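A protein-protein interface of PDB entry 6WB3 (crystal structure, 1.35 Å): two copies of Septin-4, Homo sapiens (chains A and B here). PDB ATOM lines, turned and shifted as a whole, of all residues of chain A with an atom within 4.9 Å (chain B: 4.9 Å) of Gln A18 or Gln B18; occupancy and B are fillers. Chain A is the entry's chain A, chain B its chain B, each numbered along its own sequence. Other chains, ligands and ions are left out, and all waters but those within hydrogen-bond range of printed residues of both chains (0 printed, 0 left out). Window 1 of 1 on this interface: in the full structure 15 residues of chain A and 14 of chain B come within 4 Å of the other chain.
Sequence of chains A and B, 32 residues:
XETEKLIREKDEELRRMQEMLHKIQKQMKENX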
ATOM      1  N   ASP A  11      13.249  -1.858  20.572  1.00  0.00           N
ATOM      2  CA  ASP A  11      14.590  -2.005  20.002  1.00  0.00           C
ATOM      3  C   ASP A  11      15.314  -0.650  20.030  1.00  0.00           C
ATOM      4  O   ASP A  11      16.495  -0.597  20.391  1.00  0.00           O
ATOM      5  CB  ASP A  11      14.490  -2.535  18.565  1.00  0.00           C
ATOM      6  CG  ASP A  11      15.694  -3.304  18.072  1.00  0.00           C
ATOM      7  OD1 ASP A  11      16.620  -3.540  18.872  1.00  0.00           O
ATOM      8  OD2 ASP A  11      15.714  -3.673  16.877  1.00  0.00           O
ATOM      9  N   LEU A  14      16.496   0.127  23.525  1.00  0.00           N
ATOM     10  CA  LEU A  14      17.704  -0.641  23.856  1.00  0.00           C
ATOM     11  C   LEU A  14      18.930  -0.023  23.192  1.00  0.00           C
ATOM     12  O   LEU A  14      19.989   0.040  23.830  1.00  0.00           O
ATOM     13  CB  LEU A  14      17.526  -2.081  23.428  1.00  0.00           C
ATOM     14  CG  LEU A  14      16.450  -2.825  24.194  1.00  0.00           C
ATOM     15  CD1 LEU A  14      16.154  -4.131  23.548  1.00  0.00           C
ATOM     16  CD2 LEU A  14      16.850  -3.006  25.674  1.00  0.00           C
ATOM     17  N   ARG A  15      18.804   0.491  21.958  1.00  0.00           N
ATOM     18  CA  ARG A  15      19.909   1.173  21.299  1.00  0.00           C
ATOM     19  C   ARG A  15      20.257   2.440  22.056  1.00  0.00           C
ATOM     20  O   ARG A  15      21.436   2.714  22.237  1.00  0.00           O
ATOM     21  CB  ARG A  15      19.489   1.528  19.869  1.00  0.00           C
ATOM     22  CG  ARG A  15      19.350   0.324  19.001  1.00  0.00           C
ATOM     23  CD  ARG A  15      19.425   0.683  17.536  1.00  0.00           C
ATOM     24  NE  ARG A  15      18.263   1.474  17.124  1.00  0.00           N
ATOM     25  CZ  ARG A  15      17.107   0.961  16.722  1.00  0.00           C
ATOM     26  NH1 ARG A  15      16.929  -0.354  16.700  1.00  0.00           N
ATOM     27  NH2 ARG A  15      16.113   1.757  16.360  1.00  0.00           N
ATOM     28  N   ARG A  16      19.273   3.223  22.513  1.00  0.00           N
ATOM     29  CA  ARG A  16      19.542   4.446  23.266  1.00  0.00           C
ATOM     30  C   ARG A  16      20.203   4.140  24.588  1.00  0.00           C
ATOM     31  O   ARG A  16      21.046   4.927  25.035  1.00  0.00           O
ATOM     32  CB  ARG A  16      18.271   5.264  23.509  1.00  0.00           C
ATOM     33  CG  ARG A  16      17.547   5.700  22.258  1.00  0.00           C
ATOM     34  CD  ARG A  16      18.177   6.876  21.552  1.00  0.00           C
ATOM     35  NE  ARG A  16      19.395   6.504  20.832  1.00  0.00           N
ATOM     36  CZ  ARG A  16      19.422   6.005  19.601  1.00  0.00           C
ATOM     37  NH1 ARG A  16      20.577   5.682  19.036  1.00  0.00           N
ATOM     38  NH2 ARG A  16      18.295   5.816  18.930  1.00  0.00           N
ATOM     39  N   MET A  17      19.843   3.031  25.223  1.00  0.00           N
ATOM     40  CA  MET A  17      20.469   2.622  26.470  1.00  0.00           C
ATOM     41  C   MET A  17      21.934   2.258  26.207  1.00  0.00           C
ATOM     42  O   MET A  17      22.803   2.678  26.997  1.00  0.00           O
ATOM     43  CB  MET A  17      19.704   1.442  27.086  1.00  0.00           C
ATOM     44  CG  MET A  17      18.343   1.852  27.590  1.00  0.00           C
ATOM     45  SD  MET A  17      17.234   0.451  27.898  1.00  0.00           S
ATOM     46  CE  MET A  17      17.852   0.024  29.403  1.00  0.00           C
ATOM     47  N   GLN A  18      22.229   1.580  25.089  1.00  0.00           N
ATOM     48  CA  GLN A  18      23.619   1.260  24.776  1.00  0.00           C
ATOM     49  C   GLN A  18      24.420   2.515  24.475  1.00  0.00           C
ATOM     50  O   GLN A  18      25.582   2.612  24.878  1.00  0.00           O
ATOM     51  CB  GLN A  18      23.677   0.309  23.596  1.00  0.00           C
ATOM     52  CG  GLN A  18      23.135  -1.033  24.003  1.00  0.00           C
ATOM     53  CD  GLN A  18      23.054  -2.019  22.902  1.00  0.00           C
ATOM     54  OE1 GLN A  18      24.053  -2.523  22.398  1.00  0.00           O
ATOM     55  NE2 GLN A  18      21.836  -2.369  22.577  1.00  0.00           N
ATOM     56  N   GLU A  19      23.778   3.517  23.791  1.00  0.00           N
ATOM     57  CA  GLU A  19      24.435   4.786  23.469  1.00  0.00           C
ATOM     58  C   GLU A  19      24.857   5.488  24.763  1.00  0.00           C
ATOM     59  O   GLU A  19      25.968   6.004  24.857  1.00  0.00           O
ATOM     60  CB  GLU A  19      23.466   5.671  22.643  1.00  0.00           C
ATOM     61  CG  GLU A  19      23.919   7.113  22.450  1.00  0.00           C
ATOM     62  CD  GLU A  19      22.911   8.015  21.752  1.00  0.00           C
ATOM     63  OE1 GLU A  19      21.983   7.476  21.111  1.00  0.00           O
ATOM     64  OE2 GLU A  19      23.062   9.257  21.828  1.00  0.00           O
ATOM     65  N   MET A  20      24.011   5.454  25.772  1.00  0.00           N
ATOM     66  CA  MET A  20      24.323   6.052  27.047  1.00  0.00           C
ATOM     67  C   MET A  20      25.487   5.328  27.717  1.00  0.00           C
ATOM     68  O   MET A  20      26.374   5.974  28.224  1.00  0.00           O
ATOM     69  CB  MET A  20      23.123   6.000  27.983  1.00  0.00           C
ATOM     70  CG  MET A  20      23.459   6.592  29.340  1.00  0.00           C
ATOM     71  SD  MET A  20      22.030   6.887  30.387  1.00  0.00           S
ATOM     72  CE  MET A  20      21.475   5.268  30.461  1.00  0.00           C
ATOM     73  N   LEU A  21      25.460   4.019  27.725  1.00  0.00           N
ATOM     74  CA  LEU A  21      26.570   3.258  28.323  1.00  0.00           C
ATOM     75  C   LEU A  21      27.870   3.531  27.599  1.00  0.00           C
ATOM     76  O   LEU A  21      28.902   3.688  28.252  1.00  0.00           O
ATOM     77  CB  LEU A  21      26.316   1.774  28.359  1.00  0.00           C
ATOM     78  CG  LEU A  21      25.162   1.343  29.262  1.00  0.00           C
ATOM     79  CD1 LEU A  21      25.041  -0.139  29.298  1.00  0.00           C
ATOM     80  CD2 LEU A  21      25.256   1.963  30.685  1.00  0.00           C
ATOM     81  N   HIS A  22      27.826   3.650  26.261  1.00  0.00           N
ATOM     82  CA  HIS A  22      29.050   3.959  25.513  1.00  0.00           C
ATOM     83  C   HIS A  22      29.601   5.323  25.855  1.00  0.00           C
ATOM     84  O   HIS A  22      30.823   5.500  25.928  1.00  0.00           O
ATOM     85  CB  HIS A  22      28.875   3.810  23.996  1.00  0.00           C
ATOM     86  CG  HIS A  22      28.394   2.471  23.582  1.00  0.00           C
ATOM     87  ND1 HIS A  22      28.696   1.325  24.298  1.00  0.00           N
ATOM     88  CD2 HIS A  22      27.662   2.131  22.503  1.00  0.00           C
ATOM     89  CE1 HIS A  22      28.056   0.344  23.664  1.00  0.00           C
ATOM     90  NE2 HIS A  22      27.449   0.779  22.581  1.00  0.00           N
ATOM     91  N   ASP B  11      25.991  -3.862  28.646  1.00  0.00           N
ATOM     92  CA  ASP B  11      25.885  -3.737  27.186  1.00  0.00           C
ATOM     93  C   ASP B  11      25.586  -5.081  26.552  1.00  0.00           C
ATOM     94  O   ASP B  11      24.756  -5.157  25.638  1.00  0.00           O
ATOM     95  CB  ASP B  11      27.150  -3.147  26.568  1.00  0.00           C
ATOM     96  CG  ASP B  11      27.155  -1.650  26.507  1.00  0.00           C
ATOM     97  OD1 ASP B  11      26.062  -1.061  26.412  1.00  0.00           O
ATOM     98  OD2 ASP B  11      28.264  -1.056  26.549  1.00  0.00           O
ATOM     99  N   LEU B  14      21.957  -5.865  26.967  1.00  0.00           N
ATOM    100  CA  LEU B  14      21.128  -5.085  26.054  1.00  0.00           C
ATOM    101  C   LEU B  14      21.184  -5.705  24.662  1.00  0.00           C
ATOM    102  O   LEU B  14      20.148  -5.811  23.986  1.00  0.00           O
ATOM    103  CB  LEU B  14      21.582  -3.631  26.046  1.00  0.00           C
ATOM    104  CG  LEU B  14      21.361  -2.890  27.375  1.00  0.00           C
ATOM    105  CD1 LEU B  14      22.070  -1.557  27.364  1.00  0.00           C
ATOM    106  CD2 LEU B  14      19.864  -2.732  27.692  1.00  0.00           C
ATOM    107  N   ARG B  15      22.363  -6.177  24.225  1.00  0.00           N
ATOM    108  CA  ARG B  15      22.446  -6.871  22.941  1.00  0.00           C
ATOM    109  C   ARG B  15      21.642  -8.167  22.964  1.00  0.00           C
ATOM    110  O   ARG B  15      21.037  -8.494  21.932  1.00  0.00           O
ATOM    111  CB  ARG B  15      23.910  -7.151  22.571  1.00  0.00           C
ATOM    112  CG  ARG B  15      24.706  -5.891  22.288  1.00  0.00           C
ATOM    113  CD  ARG B  15      26.048  -6.168  21.648  1.00  0.00           C
ATOM    114  NE  ARG B  15      26.937  -6.948  22.515  1.00  0.00           N
ATOM    115  CZ  ARG B  15      27.784  -6.414  23.386  1.00  0.00           C
ATOM    116  NH1 ARG B  15      27.849  -5.100  23.539  1.00  0.00           N
ATOM    117  NH2 ARG B  15      28.573  -7.192  24.110  1.00  0.00           N
ATOM    118  N   ARG B  16      21.634  -8.940  24.068  1.00  0.00           N
ATOM    119  CA  ARG B  16      20.843 -10.173  24.112  1.00  0.00           C
ATOM    120  C   ARG B  16      19.351  -9.835  24.075  1.00  0.00           C
ATOM    121  O   ARG B  16      18.584 -10.596  23.495  1.00  0.00           O
ATOM    122  CB  ARG B  16      21.150 -11.026  25.352  1.00  0.00           C
ATOM    123  CG  ARG B  16      22.585 -11.515  25.482  1.00  0.00           C
ATOM    124  CD  ARG B  16      22.977 -12.654  24.549  1.00  0.00           C
ATOM    125  NE  ARG B  16      23.021 -12.233  23.155  1.00  0.00           N
ATOM    126  CZ  ARG B  16      24.013 -11.545  22.598  1.00  0.00           C
ATOM    127  NH1 ARG B  16      25.081 -11.209  23.312  1.00  0.00           N
ATOM    128  NH2 ARG B  16      23.949 -11.199  21.319  1.00  0.00           N
ATOM    129  N   MET B  17      18.934  -8.720  24.691  1.00  0.00           N
ATOM    130  CA  MET B  17      17.546  -8.301  24.636  1.00  0.00           C
ATOM    131  C   MET B  17      17.162  -7.924  23.196  1.00  0.00           C
ATOM    132  O   MET B  17      16.084  -8.328  22.714  1.00  0.00           O
ATOM    133  CB  MET B  17      17.353  -7.131  25.593  1.00  0.00           C
ATOM    134  CG  MET B  17      17.400  -7.574  27.044  1.00  0.00           C
ATOM    135  SD  MET B  17      17.620  -6.198  28.190  1.00  0.00           S
ATOM    136  CE  MET B  17      16.005  -5.669  28.256  1.00  0.00           C
ATOM    137  N   GLN B  18      18.066  -7.273  22.464  1.00  0.00           N
ATOM    138  CA  GLN B  18      17.798  -6.943  21.071  1.00  0.00           C
ATOM    139  C   GLN B  18      17.693  -8.193  20.215  1.00  0.00           C
ATOM    140  O   GLN B  18      16.815  -8.270  19.354  1.00  0.00           O
ATOM    141  CB  GLN B  18      18.889  -6.048  20.529  1.00  0.00           C
ATOM    142  CG  GLN B  18      18.836  -4.677  21.119  1.00  0.00           C
ATOM    143  CD  GLN B  18      19.949  -3.899  20.509  1.00  0.00           C
ATOM    144  OE1 GLN B  18      21.127  -4.286  20.574  1.00  0.00           O
ATOM    145  NE2 GLN B  18      19.597  -2.816  19.872  1.00  0.00           N
ATOM    146  N   GLU B  19      18.570  -9.204  20.485  1.00  0.00           N
ATOM    147  CA  GLU B  19      18.552 -10.463  19.743  1.00  0.00           C
ATOM    148  C   GLU B  19      17.186 -11.137  19.917  1.00  0.00           C
ATOM    149  O   GLU B  19      16.591 -11.612  18.957  1.00  0.00           O
ATOM    150  CB  GLU B  19      19.706 -11.358  20.264  1.00  0.00           C
ATOM    151  CG  GLU B  19      19.699 -12.774  19.704  1.00  0.00           C
ATOM    152  CD  GLU B  19      20.752 -13.684  20.313  1.00  0.00           C
ATOM    153  OE1 GLU B  19      21.729 -13.163  20.896  1.00  0.00           O
ATOM    154  OE2 GLU B  19      20.610 -14.921  20.196  1.00  0.00           O
ATOM    155  N   MET B  20      16.663 -11.106  21.140  1.00  0.00           N
ATOM    156  CA  MET B  20      15.354 -11.681  21.414  1.00  0.00           C
ATOM    157  C   MET B  20      14.258 -10.937  20.652  1.00  0.00           C
ATOM    158  O   MET B  20      13.396 -11.588  20.051  1.00  0.00           O
ATOM    159  CB  MET B  20      15.095 -11.599  22.913  1.00  0.00           C
ATOM    160  CG  MET B  20      13.730 -12.098  23.295  1.00  0.00           C
ATOM    161  SD  MET B  20      13.418 -12.038  25.058  1.00  0.00           S
ATOM    162  CE  MET B  20      13.385 -10.469  25.328  1.00  0.00           C
ATOM    163  N   LEU B  21      14.283  -9.601  20.649  1.00  0.00           N
ATOM    164  CA  LEU B  21      13.263  -8.849  19.903  1.00  0.00           C
ATOM    165  C   LEU B  21      13.344  -9.147  18.413  1.00  0.00           C
ATOM    166  O   LEU B  21      12.307  -9.281  17.751  1.00  0.00           O
ATOM    167  CB  LEU B  21      13.409  -7.358  20.105  1.00  0.00           C
ATOM    168  CG  LEU B  21      13.164  -6.841  21.502  1.00  0.00           C
ATOM    169  CD1 LEU B  21      13.293  -5.331  21.507  1.00  0.00           C
ATOM    170  CD2 LEU B  21      11.824  -7.369  22.110  1.00  0.00           C
ATOM    171  N   HIS B  22      14.576  -9.291  17.894  1.00  0.00           N
ATOM    172  CA  HIS B  22      14.722  -9.590  16.455  1.00  0.00           C
ATOM    173  C   HIS B  22      14.156 -10.969  16.104  1.00  0.00           C
ATOM    174  O   HIS B  22      13.528 -11.142  15.054  1.00  0.00           O
ATOM    175  CB  HIS B  22      16.167  -9.399  15.987  1.00  0.00           C
ATOM    176  CG  HIS B  22      16.671  -8.004  16.187  1.00  0.00           C
ATOM    177  ND1 HIS B  22      18.021  -7.744  16.343  1.00  0.00           N
ATOM    178  CD2 HIS B  22      15.996  -6.830  16.219  1.00  0.00           C
ATOM    179  CE1 HIS B  22      18.118  -6.435  16.517  1.00  0.00           C
ATOM    180  NE2 HIS B  22      16.930  -5.842  16.439  1.00  0.00           N
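Printed residues of chain B within 4 Å of Asp A11: Gln B18, Leu B21 and His B22.
Printed residues of chain B within 4 Å of Leu A14: Leu B14, Met B17, Gln B18 and Leu B21.
Of the printed residues of chain B, Arg A15 touches Gln B18 (3.3 Å).
Of the printed residues of chain B, Gln A18 touches Asp B11, Leu B14, Arg B15 and Gln B18.
Of the printed residues of chain A, Arg B15 touches Gln A18.
Gln B18 touches four residues of chain A.
The nearest printed residue of chain A that does not touch Gln B18 is Arg A16 (6.6 Å).
The nearest printed residue of chain A that does not touch Met B17 is Met A17 (6.1 Å).
The side-chain amide nitrogen of Gln B18 sits at hydrogen-bond distance from the side-chain carboxylate of Asp A11, 3.2 Å away.
The side-chain carboxylate (OD2) of Asp A11 is in hydrogen-bond range of a ring nitrogen (NE2) of His B22 (2.5 Å).
The side-chain amide oxygen (OE1) of Gln B18 sits at hydrogen-bond distance from the side-chain amide nitrogen (NE2) of Gln A18, at 2.9 Å.
A ring nitrogen (ND1) of His A22 lies close to the side-chain carboxylate of Asp B11 (3.3 Å).
Among the printed residues, pairs that only touch across the chains: Leu A21 with Asp B11, Arg A15 with Gln B18, Gln A18 with Arg B15, Gln A18 with Leu B14, Asp A11 with Leu B21, Leu A14 with Leu B14, Leu A14 with Gln B18, Leu A14 with Leu B21, Gln A18 with Asp B11, Leu A14 with Met B17, Met A17 with Leu B14 and Leu A21 with Leu B14.
Hydrophobic or aromatic side chains of chain A that line the printed part of chain B: Leu A14, Met A17, Leu A21 and His A22.
Among the printed residues, 16 pairs touch across the chains.
Among the printed residues, no Asp or Glu carboxylate lies within 4 Å of a Lys or Arg side-chain nitrogen of the other chain.
The side-chain carboxylate (OD2) of Asp A11 is in salt-bridge range of the guanidinium group (NH1) of Arg A15 (3.5 Å).
The backbone carbonyl oxygen (O) of Leu A14 lies within hydrogen-bond range of the side-chain amide nitrogen (NE2) of Gln A18, 3.3 Å away.
O of Gln A18 lies close to ND1 of His A22 (3.4 Å).
The backbone carbonyl oxygen of Gln B18 lies close to a ring nitrogen (ND1) of His B22 (3.3 Å).
Asp A11 touches Leu B21, and with the chains exchanged Leu A21 touches Asp B11.
Leu B14 touches its own counterpart, Leu A14.
Leu A14 touches Leu B21, and with the chains exchanged Leu A21 touches Leu B14.
Gln B18 touches its own counterpart, Gln A18.
Of the 16 pairs that touch across the chains among the printed residues, 16 have their exchanged pair printed and touching as well.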
